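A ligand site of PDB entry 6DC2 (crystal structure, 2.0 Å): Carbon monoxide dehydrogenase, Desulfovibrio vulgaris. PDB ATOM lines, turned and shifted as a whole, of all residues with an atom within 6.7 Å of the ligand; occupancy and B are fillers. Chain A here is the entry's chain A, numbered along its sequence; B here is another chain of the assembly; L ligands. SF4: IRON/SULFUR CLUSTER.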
ATOM      1  N   THR A  58       6.761 -19.323 -19.717  1.00  0.00           N
ATOM      2  CA  THR A  58       7.053 -18.255 -18.772  1.00  0.00           C
ATOM      3  C   THR A  58       5.976 -18.257 -17.703  1.00  0.00           C
ATOM      4  O   THR A  58       4.801 -18.497 -18.008  1.00  0.00           O
ATOM      5  CB  THR A  58       7.105 -16.891 -19.476  1.00  0.00           C
ATOM      6  OG1 THR A  58       7.314 -15.852 -18.500  1.00  0.00           O
ATOM      7  CG2 THR A  58       5.811 -16.615 -20.240  1.00  0.00           C
ATOM      8  N   CYS A  59       6.364 -18.023 -16.454  1.00  0.00           N
ATOM      9  CA  CYS A  59       5.398 -18.044 -15.368  1.00  0.00           C
ATOM     10  C   CYS A  59       5.565 -16.817 -14.482  1.00  0.00           C
ATOM     11  O   CYS A  59       6.688 -16.392 -14.210  1.00  0.00           O
ATOM     12  CB  CYS A  59       5.517 -19.335 -14.541  1.00  0.00           C
ATOM     13  SG  CYS A  59       4.224 -19.562 -13.290  1.00  0.00           S
ATOM     14  N   ARG A  60       4.431 -16.264 -14.055  1.00  0.00           N
ATOM     15  CA  ARG A  60       4.377 -15.077 -13.214  1.00  0.00           C
ATOM     16  C   ARG A  60       3.485 -15.302 -12.002  1.00  0.00           C
ATOM     17  O   ARG A  60       2.987 -14.339 -11.413  1.00  0.00           O
ATOM     18  CB  ARG A  60       3.820 -13.883 -14.005  1.00  0.00           C
ATOM     19  CG  ARG A  60       4.845 -12.855 -14.457  1.00  0.00           C
ATOM     20  CD  ARG A  60       4.162 -11.579 -14.989  1.00  0.00           C
ATOM     21  NE  ARG A  60       3.517 -11.776 -16.285  1.00  0.00           N
ATOM     22  CZ  ARG A  60       2.198 -11.829 -16.476  1.00  0.00           C
ATOM     23  NH1 ARG A  60       1.369 -11.712 -15.442  1.00  0.00           N
ATOM     24  NH2 ARG A  60       1.707 -12.008 -17.690  1.00  0.00           N
ATOM     25  N   ASN A  61       3.251 -16.563 -11.619  1.00  0.00           N
ATOM     26  CA  ASN A  61       2.217 -16.905 -10.645  1.00  0.00           C
ATOM     27  C   ASN A  61       2.649 -16.708  -9.191  1.00  0.00           C
ATOM     28  O   ASN A  61       1.825 -16.903  -8.305  1.00  0.00           O
ATOM     29  CB  ASN A  61       1.706 -18.332 -10.853  1.00  0.00           C
ATOM     30  CG  ASN A  61       0.880 -18.463 -12.106  1.00  0.00           C
ATOM     31  OD1 ASN A  61       0.872 -17.572 -12.949  1.00  0.00           O
ATOM     32  ND2 ASN A  61       0.188 -19.589 -12.255  1.00  0.00           N
ATOM     33  N   CYS A  62       3.910 -16.338  -8.941  1.00  0.00           N
ATOM     34  CA  CYS A  62       4.340 -15.981  -7.592  1.00  0.00           C
ATOM     35  C   CYS A  62       5.595 -15.126  -7.715  1.00  0.00           C
ATOM     36  O   CYS A  62       6.186 -15.003  -8.791  1.00  0.00           O
ATOM     37  CB  CYS A  62       4.583 -17.222  -6.724  1.00  0.00           C
ATOM     38  SG  CYS A  62       6.170 -18.023  -7.013  1.00  0.00           S
ATOM     39  N   ILE A  63       5.990 -14.519  -6.595  1.00  0.00           N
ATOM     40  CA  ILE A  63       7.155 -13.648  -6.595  1.00  0.00           C
ATOM     41  C   ILE A  63       8.429 -14.345  -6.101  1.00  0.00           C
ATOM     42  O   ILE A  63       9.428 -13.674  -5.854  1.00  0.00           O
ATOM     43  CB  ILE A  63       6.911 -12.295  -5.903  1.00  0.00           C
ATOM     44  CG1 ILE A  63       6.848 -12.468  -4.385  1.00  0.00           C
ATOM     45  CG2 ILE A  63       5.643 -11.635  -6.448  1.00  0.00           C
ATOM     46  CD1 ILE A  63       7.429 -11.298  -3.629  1.00  0.00           C
ATOM     47  N   MET A  64       8.408 -15.672  -5.957  1.00  0.00           N
ATOM     48  CA  MET A  64       9.672 -16.405  -6.070  1.00  0.00           C
ATOM     49  C   MET A  64      10.216 -16.282  -7.490  1.00  0.00           C
ATOM     50  O   MET A  64      11.440 -16.306  -7.684  1.00  0.00           O
ATOM     51  CB  MET A  64       9.504 -17.877  -5.689  1.00  0.00           C
ATOM     52  CG  MET A  64       9.100 -18.153  -4.239  1.00  0.00           C
ATOM     53  SD  MET A  64       9.602 -19.780  -3.611  1.00  0.00           S
ATOM     54  CE  MET A  64       8.853 -20.915  -4.786  1.00  0.00           C
ATOM     55  N   GLY A  65       9.325 -16.139  -8.465  1.00  0.00           N
ATOM     56  CA  GLY A  65       9.717 -15.866  -9.823  1.00  0.00           C
ATOM     57  C   GLY A  65       9.873 -14.380 -10.066  1.00  0.00           C
ATOM     58  O   GLY A  65      10.158 -13.611  -9.148  1.00  0.00           O
ATOM     59  N   PRO A  66       9.657 -13.938 -11.316  1.00  0.00           N
ATOM     60  CA  PRO A  66       9.115 -14.735 -12.430  1.00  0.00           C
ATOM     61  C   PRO A  66      10.140 -15.663 -13.098  1.00  0.00           C
ATOM     62  O   PRO A  66      11.352 -15.435 -13.006  1.00  0.00           O
ATOM     63  CB  PRO A  66       8.649 -13.661 -13.424  1.00  0.00           C
ATOM     64  CG  PRO A  66       9.601 -12.531 -13.199  1.00  0.00           C
ATOM     65  CD  PRO A  66       9.946 -12.551 -11.725  1.00  0.00           C
ATOM     66  N   CYS A  67       9.639 -16.694 -13.764  1.00  0.00           N
ATOM     67  CA  CYS A  67      10.480 -17.755 -14.296  1.00  0.00           C
ATOM     68  C   CYS A  67      10.307 -17.883 -15.801  1.00  0.00           C
ATOM     69  O   CYS A  67       9.258 -17.544 -16.362  1.00  0.00           O
ATOM     70  CB  CYS A  67      10.160 -19.102 -13.628  1.00  0.00           C
ATOM     71  SG  CYS A  67      10.271 -19.095 -11.808  1.00  0.00           S
ATOM     72  N   ARG A  68      11.358 -18.379 -16.458  1.00  0.00           N
ATOM     73  CA  ARG A  68      11.335 -18.747 -17.862  1.00  0.00           C
ATOM     74  C   ARG A  68      12.000 -20.103 -17.996  1.00  0.00           C
ATOM     75  O   ARG A  68      13.007 -20.380 -17.327  1.00  0.00           O
ATOM     76  CB  ARG A  68      12.088 -17.713 -18.715  1.00  0.00           C
ATOM     77  CG  ARG A  68      11.310 -16.411 -18.979  1.00  0.00           C
ATOM     78  CD  ARG A  68      12.256 -15.293 -19.396  1.00  0.00           C
ATOM     79  NE  ARG A  68      13.321 -15.100 -18.409  1.00  0.00           N
ATOM     80  CZ  ARG A  68      14.540 -14.640 -18.699  1.00  0.00           C
ATOM     81  NH1 ARG A  68      14.851 -14.338 -19.951  1.00  0.00           N
ATOM     82  NH2 ARG A  68      15.438 -14.492 -17.737  1.00  0.00           N
ATOM     83  N   ILE A  69      11.447 -20.952 -18.845  1.00  0.00           N
ATOM     84  CA  ILE A  69      12.008 -22.274 -19.105  1.00  0.00           C
ATOM     85  C   ILE A  69      12.756 -22.204 -20.433  1.00  0.00           C
ATOM     86  O   ILE A  69      12.156 -21.954 -21.481  1.00  0.00           O
ATOM     87  CB  ILE A  69      10.909 -23.357 -19.141  1.00  0.00           C
ATOM     88  CG1 ILE A  69      10.099 -23.348 -17.834  1.00  0.00           C
ATOM     89  CG2 ILE A  69      11.523 -24.734 -19.433  1.00  0.00           C
ATOM     90  CD1 ILE A  69      10.963 -23.410 -16.572  1.00  0.00           C
ATOM     91  N   LEU A  79      13.712 -25.697 -14.929  1.00  0.00           N
ATOM     92  CA  LEU A  79      12.589 -25.678 -14.024  1.00  0.00           C
ATOM     93  C   LEU A  79      12.406 -24.270 -13.468  1.00  0.00           C
ATOM     94  O   LEU A  79      13.343 -23.470 -13.450  1.00  0.00           O
ATOM     95  CB  LEU A  79      12.825 -26.611 -12.846  1.00  0.00           C
ATOM     96  CG  LEU A  79      13.177 -28.060 -13.168  1.00  0.00           C
ATOM     97  CD1 LEU A  79      13.586 -28.763 -11.878  1.00  0.00           C
ATOM     98  CD2 LEU A  79      11.982 -28.745 -13.794  1.00  0.00           C
ATOM     99  N   GLY A  80      11.181 -23.983 -13.020  1.00  0.00           N
ATOM    100  CA  GLY A  80      10.951 -22.799 -12.229  1.00  0.00           C
ATOM    101  C   GLY A  80      11.545 -22.926 -10.835  1.00  0.00           C
ATOM    102  O   GLY A  80      12.050 -23.975 -10.435  1.00  0.00           O
ATOM    103  N   VAL A  81      11.459 -21.818 -10.088  1.00  0.00           N
ATOM    104  CA  VAL A  81      12.059 -21.772  -8.747  1.00  0.00           C
ATOM    105  C   VAL A  81      11.370 -22.767  -7.815  1.00  0.00           C
ATOM    106  O   VAL A  81      12.022 -23.371  -6.948  1.00  0.00           O
ATOM    107  CB  VAL A  81      12.021 -20.337  -8.190  1.00  0.00           C
ATOM    108  CG1 VAL A  81      12.568 -20.291  -6.776  1.00  0.00           C
ATOM    109  CG2 VAL A  81      12.812 -19.389  -9.098  1.00  0.00           C
ATOM    110  N   CYS A  82      10.065 -22.953  -7.976  1.00  0.00           N
ATOM    111  CA  CYS A  82       9.326 -23.952  -7.209  1.00  0.00           C
ATOM    112  C   CYS A  82       9.554 -25.377  -7.693  1.00  0.00           C
ATOM    113  O   CYS A  82       9.069 -26.310  -7.041  1.00  0.00           O
ATOM    114  CB  CYS A  82       7.815 -23.654  -7.273  1.00  0.00           C
ATOM    115  SG  CYS A  82       7.103 -23.783  -8.954  1.00  0.00           S
ATOM    116  N   GLY A  83      10.258 -25.569  -8.803  1.00  0.00           N
ATOM    117  CA  GLY A  83      10.471 -26.886  -9.352  1.00  0.00           C
ATOM    118  C   GLY A  83       9.573 -27.271 -10.515  1.00  0.00           C
ATOM    119  O   GLY A  83       9.729 -28.365 -11.062  1.00  0.00           O
ATOM    120  N   ALA A  84       8.647 -26.398 -10.923  1.00  0.00           N
ATOM    121  CA  ALA A  84       7.714 -26.727 -11.990  1.00  0.00           C
ATOM    122  C   ALA A  84       8.405 -26.746 -13.343  1.00  0.00           C
ATOM    123  O   ALA A  84       9.217 -25.865 -13.655  1.00  0.00           O
ATOM    124  CB  ALA A  84       6.577 -25.699 -12.010  1.00  0.00           C
ATOM    125  N   ILE A  89       3.959 -25.555 -16.341  1.00  0.00           N
ATOM    126  CA  ILE A  89       3.861 -24.106 -16.561  1.00  0.00           C
ATOM    127  C   ILE A  89       2.982 -23.808 -17.773  1.00  0.00           C
ATOM    128  O   ILE A  89       2.094 -22.951 -17.711  1.00  0.00           O
ATOM    129  CB  ILE A  89       5.258 -23.474 -16.676  1.00  0.00           C
ATOM    130  CG1 ILE A  89       5.926 -23.435 -15.297  1.00  0.00           C
ATOM    131  CG2 ILE A  89       5.167 -22.063 -17.260  1.00  0.00           C
ATOM    132  CD1 ILE A  89       7.413 -23.157 -15.335  1.00  0.00           C
ATOM    133  N   ARG A  92      -0.719 -24.775 -16.879  1.00  0.00           N
ATOM    134  CA  ARG A  92      -1.343 -23.791 -15.995  1.00  0.00           C
ATOM    135  C   ARG A  92      -1.665 -22.505 -16.746  1.00  0.00           C
ATOM    136  O   ARG A  92      -2.720 -21.899 -16.523  1.00  0.00           O
ATOM    137  CB  ARG A  92      -0.441 -23.488 -14.803  1.00  0.00           C
ATOM    138  CG  ARG A  92      -0.316 -24.615 -13.773  1.00  0.00           C
ATOM    139  CD  ARG A  92       0.399 -24.154 -12.510  1.00  0.00           C
ATOM    140  NE  ARG A  92       1.684 -23.516 -12.797  1.00  0.00           N
ATOM    141  CZ  ARG A  92       2.699 -23.466 -11.933  1.00  0.00           C
ATOM    142  NH1 ARG A  92       2.572 -24.027 -10.728  1.00  0.00           N
ATOM    143  NH2 ARG A  92       3.834 -22.858 -12.268  1.00  0.00           N
ATOM    144  N   THR A 209      -4.048 -23.559 -10.290  1.00  0.00           N
ATOM    145  CA  THR A 209      -2.905 -22.956 -10.948  1.00  0.00           C
ATOM    146  C   THR A 209      -2.042 -22.104 -10.027  1.00  0.00           C
ATOM    147  O   THR A 209      -1.006 -21.606 -10.459  1.00  0.00           O
ATOM    148  CB  THR A 209      -3.370 -22.137 -12.172  1.00  0.00           C
ATOM    149  OG1 THR A 209      -4.412 -21.240 -11.771  1.00  0.00           O
ATOM    150  CG2 THR A 209      -3.899 -23.083 -13.251  1.00  0.00           C
ATOM    151  N   HIS A 210      -2.463 -21.911  -8.771  1.00  0.00           N
ATOM    152  CA  HIS A 210      -1.578 -21.356  -7.742  1.00  0.00           C
ATOM    153  C   HIS A 210      -0.339 -22.242  -7.619  1.00  0.00           C
ATOM    154  O   HIS A 210      -0.359 -23.426  -7.955  1.00  0.00           O
ATOM    155  CB  HIS A 210      -2.331 -21.336  -6.403  1.00  0.00           C
ATOM    156  CG  HIS A 210      -1.642 -20.565  -5.316  1.00  0.00           C
ATOM    157  ND1 HIS A 210      -0.573 -21.070  -4.608  1.00  0.00           N
ATOM    158  CD2 HIS A 210      -1.898 -19.346  -4.797  1.00  0.00           C
ATOM    159  CE1 HIS A 210      -0.183 -20.184  -3.709  1.00  0.00           C
ATOM    160  NE2 HIS A 210      -0.974 -19.131  -3.794  1.00  0.00           N
ATOM    161  N   MET A 211       0.755 -21.647  -7.153  1.00  0.00           N
ATOM    162  CA  MET A 211       1.969 -22.424  -6.887  1.00  0.00           C
ATOM    163  C   MET A 211       1.647 -23.602  -5.989  1.00  0.00           C
ATOM    164  O   MET A 211       0.985 -23.448  -4.953  1.00  0.00           O
ATOM    165  CB  MET A 211       3.040 -21.531  -6.233  1.00  0.00           C
ATOM    166  CG  MET A 211       4.476 -22.121  -6.218  1.00  0.00           C
ATOM    167  SD  MET A 211       4.744 -23.610  -5.208  1.00  0.00           S
ATOM    168  CE  MET A 211       5.636 -22.949  -3.810  1.00  0.00           C
ATOM    169  N   GLY A 212       2.099 -24.791  -6.377  1.00  0.00           N
ATOM    170  CA  GLY A 212       2.044 -25.933  -5.484  1.00  0.00           C
ATOM    171  C   GLY A 212       0.669 -26.514  -5.270  1.00  0.00           C
ATOM    172  O   GLY A 212       0.412 -27.083  -4.199  1.00  0.00           O
ATOM    173  N   GLN B  46      17.349 -18.504 -12.119  1.00  0.00           N
ATOM    174  CA  GLN B  46      16.314 -17.638 -12.666  1.00  0.00           C
ATOM    175  C   GLN B  46      16.612 -16.153 -12.468  1.00  0.00           C
ATOM    176  O   GLN B  46      15.731 -15.317 -12.724  1.00  0.00           O
ATOM    177  CB  GLN B  46      14.941 -18.005 -12.077  1.00  0.00           C
ATOM    178  CG  GLN B  46      14.452 -19.389 -12.504  1.00  0.00           C
ATOM    179  CD  GLN B  46      13.993 -19.428 -13.954  1.00  0.00           C
ATOM    180  OE1 GLN B  46      13.791 -18.379 -14.588  1.00  0.00           O
ATOM    181  NE2 GLN B  46      13.825 -20.630 -14.493  1.00  0.00           N
ATOM    182  N   PRO B 351       6.770 -28.843  -6.360  1.00  0.00           N
ATOM    183  CA  PRO B 351       6.934 -30.148  -7.044  1.00  0.00           C
ATOM    184  C   PRO B 351       8.344 -30.694  -7.001  1.00  0.00           C
ATOM    185  O   PRO B 351       8.540 -31.886  -7.257  1.00  0.00           O
ATOM    186  CB  PRO B 351       6.485 -29.855  -8.478  1.00  0.00           C
ATOM    187  CG  PRO B 351       6.594 -28.356  -8.613  1.00  0.00           C
ATOM    188  CD  PRO B 351       6.231 -27.816  -7.264  1.00  0.00           C
ATOM    189  N   TYR B 561       5.727 -14.593  -0.671  1.00  0.00           N
ATOM    190  CA  TYR B 561       5.939 -15.078  -2.034  1.00  0.00           C
ATOM    191  C   TYR B 561       4.646 -15.314  -2.818  1.00  0.00           C
ATOM    192  O   TYR B 561       4.648 -15.106  -4.033  1.00  0.00           O
ATOM    193  CB  TYR B 561       6.783 -16.373  -2.061  1.00  0.00           C
ATOM    194  CG  TYR B 561       5.943 -17.621  -2.199  1.00  0.00           C
ATOM    195  CD1 TYR B 561       5.548 -18.084  -3.453  1.00  0.00           C
ATOM    196  CD2 TYR B 561       5.494 -18.315  -1.073  1.00  0.00           C
ATOM    197  CE1 TYR B 561       4.736 -19.195  -3.596  1.00  0.00           C
ATOM    198  CE2 TYR B 561       4.680 -19.451  -1.216  1.00  0.00           C
ATOM    199  CZ  TYR B 561       4.310 -19.879  -2.486  1.00  0.00           C
ATOM    200  OH  TYR B 561       3.499 -20.982  -2.641  1.00  0.00           O
HETATM  201 FE1  SF4 L   1       5.596 -19.915 -11.505  1.00  0.00          FE
HETATM  202 FE2  SF4 L   1       8.244 -19.588 -10.898  1.00  0.00          FE
HETATM  203 FE3  SF4 L   1       6.822 -21.656  -9.771  1.00  0.00          FE
HETATM  204 FE4  SF4 L   1       6.325 -19.057  -9.017  1.00  0.00          FE
HETATM  205  S1  SF4 L   1       8.253 -20.215  -8.709  1.00  0.00           S
HETATM  206  S2  SF4 L   1       4.764 -20.666  -9.518  1.00  0.00           S
HETATM  207  S3  SF4 L   1       6.649 -17.953 -10.972  1.00  0.00           S
HETATM  208  S4  SF4 L   1       7.302 -21.351 -11.980  1.00  0.00           S
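CA of Gly 65 touches S3 of the ligand (3.9 Å). Gly 80 touches the ligand. Val 81 touches the ligand. Ile 89 touches the ligand (CD1 to S4, 3.8 Å). Met 211 touches the ligand. 11 residues have an atom within 4 Å of the ligand: Cys 59, Asn 61, Cys 62, Gly 65, Cys 67, Gly 80, Val 81, Cys 82, Ile 89, Arg 92 and Met 211. The nearest printed residue that does not touch the ligand is Met 64 (4.02 Å).
The backbone carbonyl oxygen (O) of Cys 67 lies close to the side-chain hydroxyl (OG1) of Thr 58 (3.3 Å). The side-chain sulfur of Cys 67 lies close to the backbone NH of Val 81 (3.4 Å). N of Cys 59 lies within hydrogen-bond range of O of Cys 67 (2.9 Å). SG of Cys 59 sits close to N of Asn 61 (3.6 Å). The side-chain amide nitrogen (ND2) of Asn 61 lies within hydrogen-bond range of the backbone carbonyl oxygen (O) of Thr 209. SG of Cys 82 lies close to N of Ala 84 (3.6 Å). The side-chain sulfur (SG) of Cys 62 lies close to the backbone NH (N) of Met 64 (3.4 Å). The side-chain sulfur of Cys 59 sits close to the guanidinium group of Arg 92.
A sulfur (S2) of the ligand sits close to the guanidinium group of Arg 92. N of Cys 82 sits close to S1 of the ligand. N of Asn 61 sits close to S3 of the ligand, 3.7 Å away. SG of Cys 67 binds FE2 of the ligand (2.3 Å). A sulfur (S3) of the ligand lies close to the backbone NH of Cys 62. FE1 of the ligand is bound by SG of Cys 59 (2.3 Å). SG of Cys 82 is bound to FE3 of the ligand (2.3 Å). The side-chain sulfur (SG) of Cys 62 binds an iron atom (FE4) of the ligand, at 2.3 Å.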
